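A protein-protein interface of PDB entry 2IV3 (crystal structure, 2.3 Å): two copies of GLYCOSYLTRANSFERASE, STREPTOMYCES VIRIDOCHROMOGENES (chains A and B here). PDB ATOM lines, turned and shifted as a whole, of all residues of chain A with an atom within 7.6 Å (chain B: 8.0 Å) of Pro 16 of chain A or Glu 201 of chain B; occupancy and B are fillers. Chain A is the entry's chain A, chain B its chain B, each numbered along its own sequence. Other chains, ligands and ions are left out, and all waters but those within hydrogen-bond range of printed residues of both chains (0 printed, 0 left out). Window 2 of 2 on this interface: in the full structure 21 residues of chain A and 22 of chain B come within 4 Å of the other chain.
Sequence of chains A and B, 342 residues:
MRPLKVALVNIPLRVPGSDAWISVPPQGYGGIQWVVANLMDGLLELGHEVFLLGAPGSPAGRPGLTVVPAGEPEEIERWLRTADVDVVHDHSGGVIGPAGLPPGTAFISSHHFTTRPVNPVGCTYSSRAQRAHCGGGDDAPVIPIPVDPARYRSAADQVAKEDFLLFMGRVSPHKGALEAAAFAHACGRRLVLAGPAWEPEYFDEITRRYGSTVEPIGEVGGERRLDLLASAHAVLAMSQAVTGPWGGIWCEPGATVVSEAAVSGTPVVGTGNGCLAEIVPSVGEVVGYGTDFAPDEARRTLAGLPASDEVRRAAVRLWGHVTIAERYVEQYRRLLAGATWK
O of Trp 198 of chain B lies close to O of Trp 198 of chain A, at 3.0 Å.
The guanidinium group of Arg 208 of chain B lies close to the backbone carbonyl oxygen of Asp 204 of chain B, 3.4 Å away.
Among the printed residues, merely in contact across the chains: Pro 16 of chain A with Glu 201 of chain B, Gly 17 of chain A with Glu 201 of chain B, Gly 17 of chain A with Glu 205 of chain B, Gly 17 of chain A with Arg 208 of chain B, Trp 198 of chain A with Pro 200 of chain B and Trp 198 of chain A with Glu 201 of chain B.
Pro 16 of chain A touches just one residue of chain B: Glu 201.
Of the printed residues of chain B, Gly 17 of chain A touches Glu 201 (3.8 Å), Glu 205 (3.7 Å) and Arg 208 (3.6 Å).
Of the printed residues of chain A, Trp 198 of chain B touches Trp 198.
Of the printed residues of chain A, Arg 208 of chain B touches Gly 17.
The nearest residue of chain A that does not touch Glu 201 of chain B is Glu 219 of chain A (5.5 Å).
The nearest printed residue of chain A that does not touch Arg 208 of chain B is Ser 18 of chain A (5.8 Å).
Hydrophobic or aromatic side chains of chain B that line the printed part of chain A: Trp 198 and Pro 200.
Printed residues of chain A that touch a printed residue of chain B: Pro 16, Gly 17 and Trp 198.
Hydrophobic or aromatic side chains of chain A that line the printed part of chain B: Pro 16 and Trp 198.
Trp 198 of chain A touches its own counterpart, Trp 198 of chain B.
Of the 7 pairs that touch across the chains among the printed residues, 1 has its exchanged pair printed and touching as well.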
ATOM      1  N   LEU A  13     -21.047   4.259  33.829  1.00  0.00           N
ATOM      2  CA  LEU A  13     -21.368   3.483  32.635  1.00  0.00           C
ATOM      3  C   LEU A  13     -22.646   4.011  32.011  1.00  0.00           C
ATOM      4  O   LEU A  13     -23.624   4.286  32.696  1.00  0.00           O
ATOM      5  CB  LEU A  13     -21.561   1.981  32.961  1.00  0.00           C
ATOM      6  CG  LEU A  13     -20.437   1.157  33.614  1.00  0.00           C
ATOM      7  CD1 LEU A  13     -21.012  -0.181  34.045  1.00  0.00           C
ATOM      8  CD2 LEU A  13     -19.230   0.951  32.709  1.00  0.00           C
ATOM      9  N   ARG A  14     -22.629   4.144  30.698  1.00  0.00           N
ATOM     10  CA  ARG A  14     -23.818   4.585  29.998  1.00  0.00           C
ATOM     11  C   ARG A  14     -24.713   3.387  29.782  1.00  0.00           C
ATOM     12  O   ARG A  14     -24.242   2.227  29.698  1.00  0.00           O
ATOM     13  CB  ARG A  14     -23.469   5.222  28.662  1.00  0.00           C
ATOM     14  CG  ARG A  14     -22.424   6.295  28.756  1.00  0.00           C
ATOM     15  CD  ARG A  14     -23.060   7.669  28.646  1.00  0.00           C
ATOM     16  NE  ARG A  14     -22.068   8.720  28.438  1.00  0.00           N
ATOM     17  CZ  ARG A  14     -22.324  10.024  28.498  1.00  0.00           C
ATOM     18  NH1 ARG A  14     -23.543  10.480  28.773  1.00  0.00           N
ATOM     19  NH2 ARG A  14     -21.342  10.884  28.297  1.00  0.00           N
ATOM     20  N   VAL A  15     -26.009   3.678  29.711  1.00  0.00           N
ATOM     21  CA  VAL A  15     -27.006   2.738  29.256  1.00  0.00           C
ATOM     22  C   VAL A  15     -26.652   2.433  27.807  1.00  0.00           C
ATOM     23  O   VAL A  15     -26.361   3.364  27.035  1.00  0.00           O
ATOM     24  CB  VAL A  15     -28.378   3.384  29.342  1.00  0.00           C
ATOM     25  CG1 VAL A  15     -29.416   2.562  28.593  1.00  0.00           C
ATOM     26  CG2 VAL A  15     -28.744   3.580  30.797  1.00  0.00           C
ATOM     27  N   PRO A  16     -26.617   1.135  27.442  1.00  0.00           N
ATOM     28  CA  PRO A  16     -26.158   0.696  26.111  1.00  0.00           C
ATOM     29  C   PRO A  16     -26.926   1.278  24.925  1.00  0.00           C
ATOM     30  O   PRO A  16     -28.144   1.117  24.810  1.00  0.00           O
ATOM     31  CB  PRO A  16     -26.315  -0.831  26.185  1.00  0.00           C
ATOM     32  CG  PRO A  16     -26.168  -1.132  27.649  1.00  0.00           C
ATOM     33  CD  PRO A  16     -26.940  -0.023  28.300  1.00  0.00           C
ATOM     34  N   GLY A  17     -26.209   1.939  24.033  1.00  0.00           N
ATOM     35  CA  GLY A  17     -26.832   2.610  22.914  1.00  0.00           C
ATOM     36  C   GLY A  17     -27.552   3.900  23.239  1.00  0.00           C
ATOM     37  O   GLY A  17     -28.202   4.461  22.385  1.00  0.00           O
ATOM     38  N   SER A  18     -27.438   4.369  24.471  1.00  0.00           N
ATOM     39  CA  SER A  18     -27.982   5.659  24.865  1.00  0.00           C
ATOM     40  C   SER A  18     -26.934   6.522  25.542  1.00  0.00           C
ATOM     41  O   SER A  18     -25.848   6.058  25.871  1.00  0.00           O
ATOM     42  CB  SER A  18     -29.170   5.482  25.798  1.00  0.00           C
ATOM     43  OG  SER A  18     -29.084   6.337  26.907  1.00  0.00           O
ATOM     44  N   ASP A  19     -27.277   7.783  25.749  1.00  0.00           N
ATOM     45  CA  ASP A  19     -26.352   8.739  26.308  1.00  0.00           C
ATOM     46  C   ASP A  19     -26.514   8.786  27.814  1.00  0.00           C
ATOM     47  O   ASP A  19     -25.590   9.141  28.532  1.00  0.00           O
ATOM     48  CB  ASP A  19     -26.595  10.126  25.723  1.00  0.00           C
ATOM     49  CG  ASP A  19     -25.763  10.394  24.494  1.00  0.00           C
ATOM     50  OD1 ASP A  19     -24.630   9.882  24.398  1.00  0.00           O
ATOM     51  OD2 ASP A  19     -26.254  11.119  23.613  1.00  0.00           O
ATOM     52  N   ALA A  20     -27.706   8.418  28.268  1.00  0.00           N
ATOM     53  CA  ALA A  20     -28.047   8.399  29.680  1.00  0.00           C
ATOM     54  C   ALA A  20     -27.256   7.380  30.483  1.00  0.00           C
ATOM     55  O   ALA A  20     -26.732   6.424  29.943  1.00  0.00           O
ATOM     56  CB  ALA A  20     -29.507   8.190  29.861  1.00  0.00           C
ATOM     57  N   TRP A  21     -27.183   7.620  31.782  1.00  0.00           N
ATOM     58  CA  TRP A  21     -26.391   6.827  32.706  1.00  0.00           C
ATOM     59  C   TRP A  21     -27.186   5.669  33.355  1.00  0.00           C
ATOM     60  O   TRP A  21     -28.410   5.722  33.486  1.00  0.00           O
ATOM     61  CB  TRP A  21     -25.730   7.733  33.764  1.00  0.00           C
ATOM     62  CG  TRP A  21     -24.772   8.704  33.148  1.00  0.00           C
ATOM     63  CD1 TRP A  21     -25.069   9.961  32.657  1.00  0.00           C
ATOM     64  CD2 TRP A  21     -23.381   8.506  32.906  1.00  0.00           C
ATOM     65  NE1 TRP A  21     -23.952  10.541  32.129  1.00  0.00           N
ATOM     66  CE2 TRP A  21     -22.895   9.684  32.274  1.00  0.00           C
ATOM     67  CE3 TRP A  21     -22.489   7.460  33.165  1.00  0.00           C
ATOM     68  CZ2 TRP A  21     -21.563   9.842  31.910  1.00  0.00           C
ATOM     69  CZ3 TRP A  21     -21.156   7.619  32.794  1.00  0.00           C
ATOM     70  CH2 TRP A  21     -20.706   8.803  32.178  1.00  0.00           C
ATOM     71  N   ILE A  22     -26.473   4.602  33.697  1.00  0.00           N
ATOM     72  CA  ILE A  22     -27.037   3.520  34.450  1.00  0.00           C
ATOM     73  C   ILE A  22     -27.085   4.034  35.890  1.00  0.00           C
ATOM     74  O   ILE A  22     -26.073   4.517  36.461  1.00  0.00           O
ATOM     75  CB  ILE A  22     -26.181   2.241  34.345  1.00  0.00           C
ATOM     76  CG1 ILE A  22     -26.392   1.549  33.003  1.00  0.00           C
ATOM     77  CG2 ILE A  22     -26.509   1.279  35.478  1.00  0.00           C
ATOM     78  CD1 ILE A  22     -25.238   0.650  32.606  1.00  0.00           C
ATOM     79  N   PRO A 196     -28.868 -10.678  30.447  1.00  0.00           N
ATOM     80  CA  PRO A 196     -28.294 -10.359  29.130  1.00  0.00           C
ATOM     81  C   PRO A 196     -27.637 -11.592  28.507  1.00  0.00           C
ATOM     82  O   PRO A 196     -26.788 -12.250  29.144  1.00  0.00           O
ATOM     83  CB  PRO A 196     -27.226  -9.310  29.438  1.00  0.00           C
ATOM     84  CG  PRO A 196     -27.561  -8.769  30.761  1.00  0.00           C
ATOM     85  CD  PRO A 196     -28.296  -9.842  31.517  1.00  0.00           C
ATOM     86  N   TRP A 198     -25.381 -11.734  25.831  1.00  0.00           N
ATOM     87  CA  TRP A 198     -24.604 -10.988  24.843  1.00  0.00           C
ATOM     88  C   TRP A 198     -23.794 -11.859  23.852  1.00  0.00           C
ATOM     89  O   TRP A 198     -23.427 -11.407  22.768  1.00  0.00           O
ATOM     90  CB  TRP A 198     -23.888  -9.772  25.458  1.00  0.00           C
ATOM     91  CG  TRP A 198     -24.870  -8.606  25.518  1.00  0.00           C
ATOM     92  CD1 TRP A 198     -26.165  -8.601  25.026  1.00  0.00           C
ATOM     93  CD2 TRP A 198     -24.642  -7.291  26.034  1.00  0.00           C
ATOM     94  NE1 TRP A 198     -26.747  -7.373  25.229  1.00  0.00           N
ATOM     95  CE2 TRP A 198     -25.834  -6.548  25.843  1.00  0.00           C
ATOM     96  CE3 TRP A 198     -23.540  -6.659  26.643  1.00  0.00           C
ATOM     97  CZ2 TRP A 198     -25.961  -5.199  26.233  1.00  0.00           C
ATOM     98  CZ3 TRP A 198     -23.666  -5.300  27.035  1.00  0.00           C
ATOM     99  CH2 TRP A 198     -24.874  -4.595  26.824  1.00  0.00           C
ATOM    100  N   GLU A 219     -32.835  -9.808  30.004  1.00  0.00           N
ATOM    101  CA  GLU A 219     -32.570  -8.947  31.152  1.00  0.00           C
ATOM    102  C   GLU A 219     -33.852  -8.622  31.913  1.00  0.00           C
ATOM    103  O   GLU A 219     -34.909  -8.467  31.314  1.00  0.00           O
ATOM    104  CB  GLU A 219     -31.907  -7.644  30.702  1.00  0.00           C
ATOM    105  CG  GLU A 219     -31.060  -6.994  31.823  1.00  0.00           C
ATOM    106  CD  GLU A 219     -30.136  -5.859  31.352  1.00  0.00           C
ATOM    107  OE1 GLU A 219     -29.386  -6.040  30.370  1.00  0.00           O
ATOM    108  OE2 GLU A 219     -30.121  -4.787  32.000  1.00  0.00           O
ATOM    109  N   PRO B 173     -17.667  -0.275  22.584  1.00  0.00           N
ATOM    110  CA  PRO B 173     -17.427   1.149  22.846  1.00  0.00           C
ATOM    111  C   PRO B 173     -15.961   1.551  23.086  1.00  0.00           C
ATOM    112  O   PRO B 173     -15.556   2.647  22.705  1.00  0.00           O
ATOM    113  CB  PRO B 173     -18.299   1.422  24.090  1.00  0.00           C
ATOM    114  CG  PRO B 173     -19.464   0.443  23.927  1.00  0.00           C
ATOM    115  CD  PRO B 173     -18.741  -0.807  23.451  1.00  0.00           C
ATOM    116  N   TRP B 198     -21.537  -8.103  19.366  1.00  0.00           N
ATOM    117  CA  TRP B 198     -22.169  -8.884  20.429  1.00  0.00           C
ATOM    118  C   TRP B 198     -23.006  -7.994  21.324  1.00  0.00           C
ATOM    119  O   TRP B 198     -23.864  -8.474  22.091  1.00  0.00           O
ATOM    120  CB  TRP B 198     -21.092  -9.635  21.244  1.00  0.00           C
ATOM    121  CG  TRP B 198     -20.589 -10.879  20.537  1.00  0.00           C
ATOM    122  CD1 TRP B 198     -20.813 -11.237  19.214  1.00  0.00           C
ATOM    123  CD2 TRP B 198     -19.743 -11.896  21.079  1.00  0.00           C
ATOM    124  NE1 TRP B 198     -20.162 -12.415  18.922  1.00  0.00           N
ATOM    125  CE2 TRP B 198     -19.509 -12.848  20.046  1.00  0.00           C
ATOM    126  CE3 TRP B 198     -19.170 -12.113  22.342  1.00  0.00           C
ATOM    127  CZ2 TRP B 198     -18.734 -14.011  20.248  1.00  0.00           C
ATOM    128  CZ3 TRP B 198     -18.393 -13.280  22.546  1.00  0.00           C
ATOM    129  CH2 TRP B 198     -18.181 -14.208  21.501  1.00  0.00           C
ATOM    130  N   GLU B 199     -22.781  -6.691  21.201  1.00  0.00           N
ATOM    131  CA  GLU B 199     -23.502  -5.704  21.999  1.00  0.00           C
ATOM    132  C   GLU B 199     -24.515  -5.003  21.107  1.00  0.00           C
ATOM    133  O   GLU B 199     -24.174  -4.051  20.392  1.00  0.00           O
ATOM    134  CB  GLU B 199     -22.493  -4.760  22.665  1.00  0.00           C
ATOM    135  CG  GLU B 199     -21.220  -5.526  22.999  1.00  0.00           C
ATOM    136  CD  GLU B 199     -20.161  -4.737  23.736  1.00  0.00           C
ATOM    137  OE1 GLU B 199     -20.482  -3.725  24.384  1.00  0.00           O
ATOM    138  OE2 GLU B 199     -19.000  -5.168  23.682  1.00  0.00           O
ATOM    139  N   PRO B 200     -25.766  -5.496  21.121  1.00  0.00           N
ATOM    140  CA  PRO B 200     -26.802  -5.149  20.124  1.00  0.00           C
ATOM    141  C   PRO B 200     -27.172  -3.669  20.086  1.00  0.00           C
ATOM    142  O   PRO B 200     -27.215  -3.067  19.002  1.00  0.00           O
ATOM    143  CB  PRO B 200     -28.013  -5.988  20.549  1.00  0.00           C
ATOM    144  CG  PRO B 200     -27.482  -7.048  21.401  1.00  0.00           C
ATOM    145  CD  PRO B 200     -26.294  -6.435  22.120  1.00  0.00           C
ATOM    146  N   GLU B 201     -27.420  -3.093  21.259  1.00  0.00           N
ATOM    147  CA  GLU B 201     -27.794  -1.694  21.385  1.00  0.00           C
ATOM    148  C   GLU B 201     -26.745  -0.740  20.766  1.00  0.00           C
ATOM    149  O   GLU B 201     -27.111   0.146  20.004  1.00  0.00           O
ATOM    150  CB  GLU B 201     -28.104  -1.377  22.856  1.00  0.00           C
ATOM    151  CG  GLU B 201     -29.218  -2.286  23.471  1.00  0.00           C
ATOM    152  CD  GLU B 201     -28.729  -3.387  24.456  1.00  0.00           C
ATOM    153  OE1 GLU B 201     -27.630  -3.995  24.234  1.00  0.00           O
ATOM    154  OE2 GLU B 201     -29.462  -3.642  25.466  1.00  0.00           O
ATOM    155  N   TYR B 202     -25.459  -0.942  21.080  1.00  0.00           N
ATOM    156  CA  TYR B 202     -24.357  -0.123  20.533  1.00  0.00           C
ATOM    157  C   TYR B 202     -24.207  -0.286  19.017  1.00  0.00           C
ATOM    158  O   TYR B 202     -23.930   0.687  18.309  1.00  0.00           O
ATOM    159  CB  TYR B 202     -23.039  -0.485  21.233  1.00  0.00           C
ATOM    160  CG  TYR B 202     -21.789   0.216  20.756  1.00  0.00           C
ATOM    161  CD1 TYR B 202     -21.576   1.573  21.001  1.00  0.00           C
ATOM    162  CD2 TYR B 202     -20.771  -0.511  20.109  1.00  0.00           C
ATOM    163  CE1 TYR B 202     -20.384   2.195  20.571  1.00  0.00           C
ATOM    164  CE2 TYR B 202     -19.596   0.096  19.667  1.00  0.00           C
ATOM    165  CZ  TYR B 202     -19.407   1.439  19.892  1.00  0.00           C
ATOM    166  OH  TYR B 202     -18.230   2.014  19.466  1.00  0.00           O
ATOM    167  N   PHE B 203     -24.388  -1.524  18.541  1.00  0.00           N
ATOM    168  CA  PHE B 203     -24.423  -1.826  17.115  1.00  0.00           C
ATOM    169  C   PHE B 203     -25.567  -1.062  16.482  1.00  0.00           C
ATOM    170  O   PHE B 203     -25.383  -0.400  15.462  1.00  0.00           O
ATOM    171  CB  PHE B 203     -24.605  -3.326  16.879  1.00  0.00           C
ATOM    172  CG  PHE B 203     -24.731  -3.716  15.421  1.00  0.00           C
ATOM    173  CD1 PHE B 203     -23.602  -3.989  14.663  1.00  0.00           C
ATOM    174  CD2 PHE B 203     -26.000  -3.821  14.812  1.00  0.00           C
ATOM    175  CE1 PHE B 203     -23.704  -4.363  13.324  1.00  0.00           C
ATOM    176  CE2 PHE B 203     -26.132  -4.181  13.471  1.00  0.00           C
ATOM    177  CZ  PHE B 203     -24.989  -4.465  12.720  1.00  0.00           C
ATOM    178  N   ASP B 204     -26.737  -1.130  17.089  1.00  0.00           N
ATOM    179  CA  ASP B 204     -27.925  -0.527  16.474  1.00  0.00           C
ATOM    180  C   ASP B 204     -27.823   0.982  16.438  1.00  0.00           C
ATOM    181  O   ASP B 204     -28.458   1.629  15.623  1.00  0.00           O
ATOM    182  CB  ASP B 204     -29.204  -0.940  17.204  1.00  0.00           C
ATOM    183  CG  ASP B 204     -29.573  -2.394  16.958  1.00  0.00           C
ATOM    184  OD1 ASP B 204     -29.120  -2.976  15.937  1.00  0.00           O
ATOM    185  OD2 ASP B 204     -30.306  -2.958  17.800  1.00  0.00           O
ATOM    186  N   GLU B 205     -26.998   1.535  17.317  1.00  0.00           N
ATOM    187  CA  GLU B 205     -26.896   2.972  17.459  1.00  0.00           C
ATOM    188  C   GLU B 205     -25.903   3.488  16.445  1.00  0.00           C
ATOM    189  O   GLU B 205     -26.075   4.564  15.902  1.00  0.00           O
ATOM    190  CB  GLU B 205     -26.488   3.316  18.893  1.00  0.00           C
ATOM    191  CG  GLU B 205     -26.324   4.800  19.222  1.00  0.00           C
ATOM    192  CD  GLU B 205     -25.206   5.008  20.246  1.00  0.00           C
ATOM    193  OE1 GLU B 205     -24.407   4.055  20.428  1.00  0.00           O
ATOM    194  OE2 GLU B 205     -25.132   6.096  20.882  1.00  0.00           O
ATOM    195  N   ILE B 206     -24.861   2.699  16.202  1.00  0.00           N
ATOM    196  CA  ILE B 206     -23.964   2.909  15.072  1.00  0.00           C
ATOM    197  C   ILE B 206     -24.779   3.017  13.775  1.00  0.00           C
ATOM    198  O   ILE B 206     -24.725   4.043  13.096  1.00  0.00           O
ATOM    199  CB  ILE B 206     -22.906   1.757  14.933  1.00  0.00           C
ATOM    200  CG1 ILE B 206     -21.936   1.763  16.114  1.00  0.00           C
ATOM    201  CG2 ILE B 206     -22.160   1.841  13.560  1.00  0.00           C
ATOM    202  CD1 ILE B 206     -21.038   0.607  16.140  1.00  0.00           C
ATOM    203  N   THR B 207     -25.531   1.964  13.444  1.00  0.00           N
ATOM    204  CA  THR B 207     -26.328   1.956  12.207  1.00  0.00           C
ATOM    205  C   THR B 207     -27.427   3.016  12.197  1.00  0.00           C
ATOM    206  O   THR B 207     -27.581   3.721  11.210  1.00  0.00           O
ATOM    207  CB  THR B 207     -26.892   0.566  11.807  1.00  0.00           C
ATOM    208  OG1 THR B 207     -28.058   0.280  12.572  1.00  0.00           O
ATOM    209  CG2 THR B 207     -25.853  -0.529  11.986  1.00  0.00           C
ATOM    210  N   ARG B 208     -28.161   3.155  13.296  1.00  0.00           N
ATOM    211  CA  ARG B 208     -29.076   4.276  13.425  1.00  0.00           C
ATOM    212  C   ARG B 208     -28.374   5.610  13.103  1.00  0.00           C
ATOM    213  O   ARG B 208     -28.886   6.407  12.328  1.00  0.00           O
ATOM    214  CB  ARG B 208     -29.715   4.300  14.811  1.00  0.00           C
ATOM    215  CG  ARG B 208     -31.125   4.928  14.880  1.00  0.00           C
ATOM    216  CD  ARG B 208     -31.857   4.619  16.222  1.00  0.00           C
ATOM    217  NE  ARG B 208     -30.962   4.696  17.392  1.00  0.00           N
ATOM    218  CZ  ARG B 208     -30.536   3.650  18.116  1.00  0.00           C
ATOM    219  NH1 ARG B 208     -30.932   2.407  17.829  1.00  0.00           N
ATOM    220  NH2 ARG B 208     -29.709   3.849  19.141  1.00  0.00           N
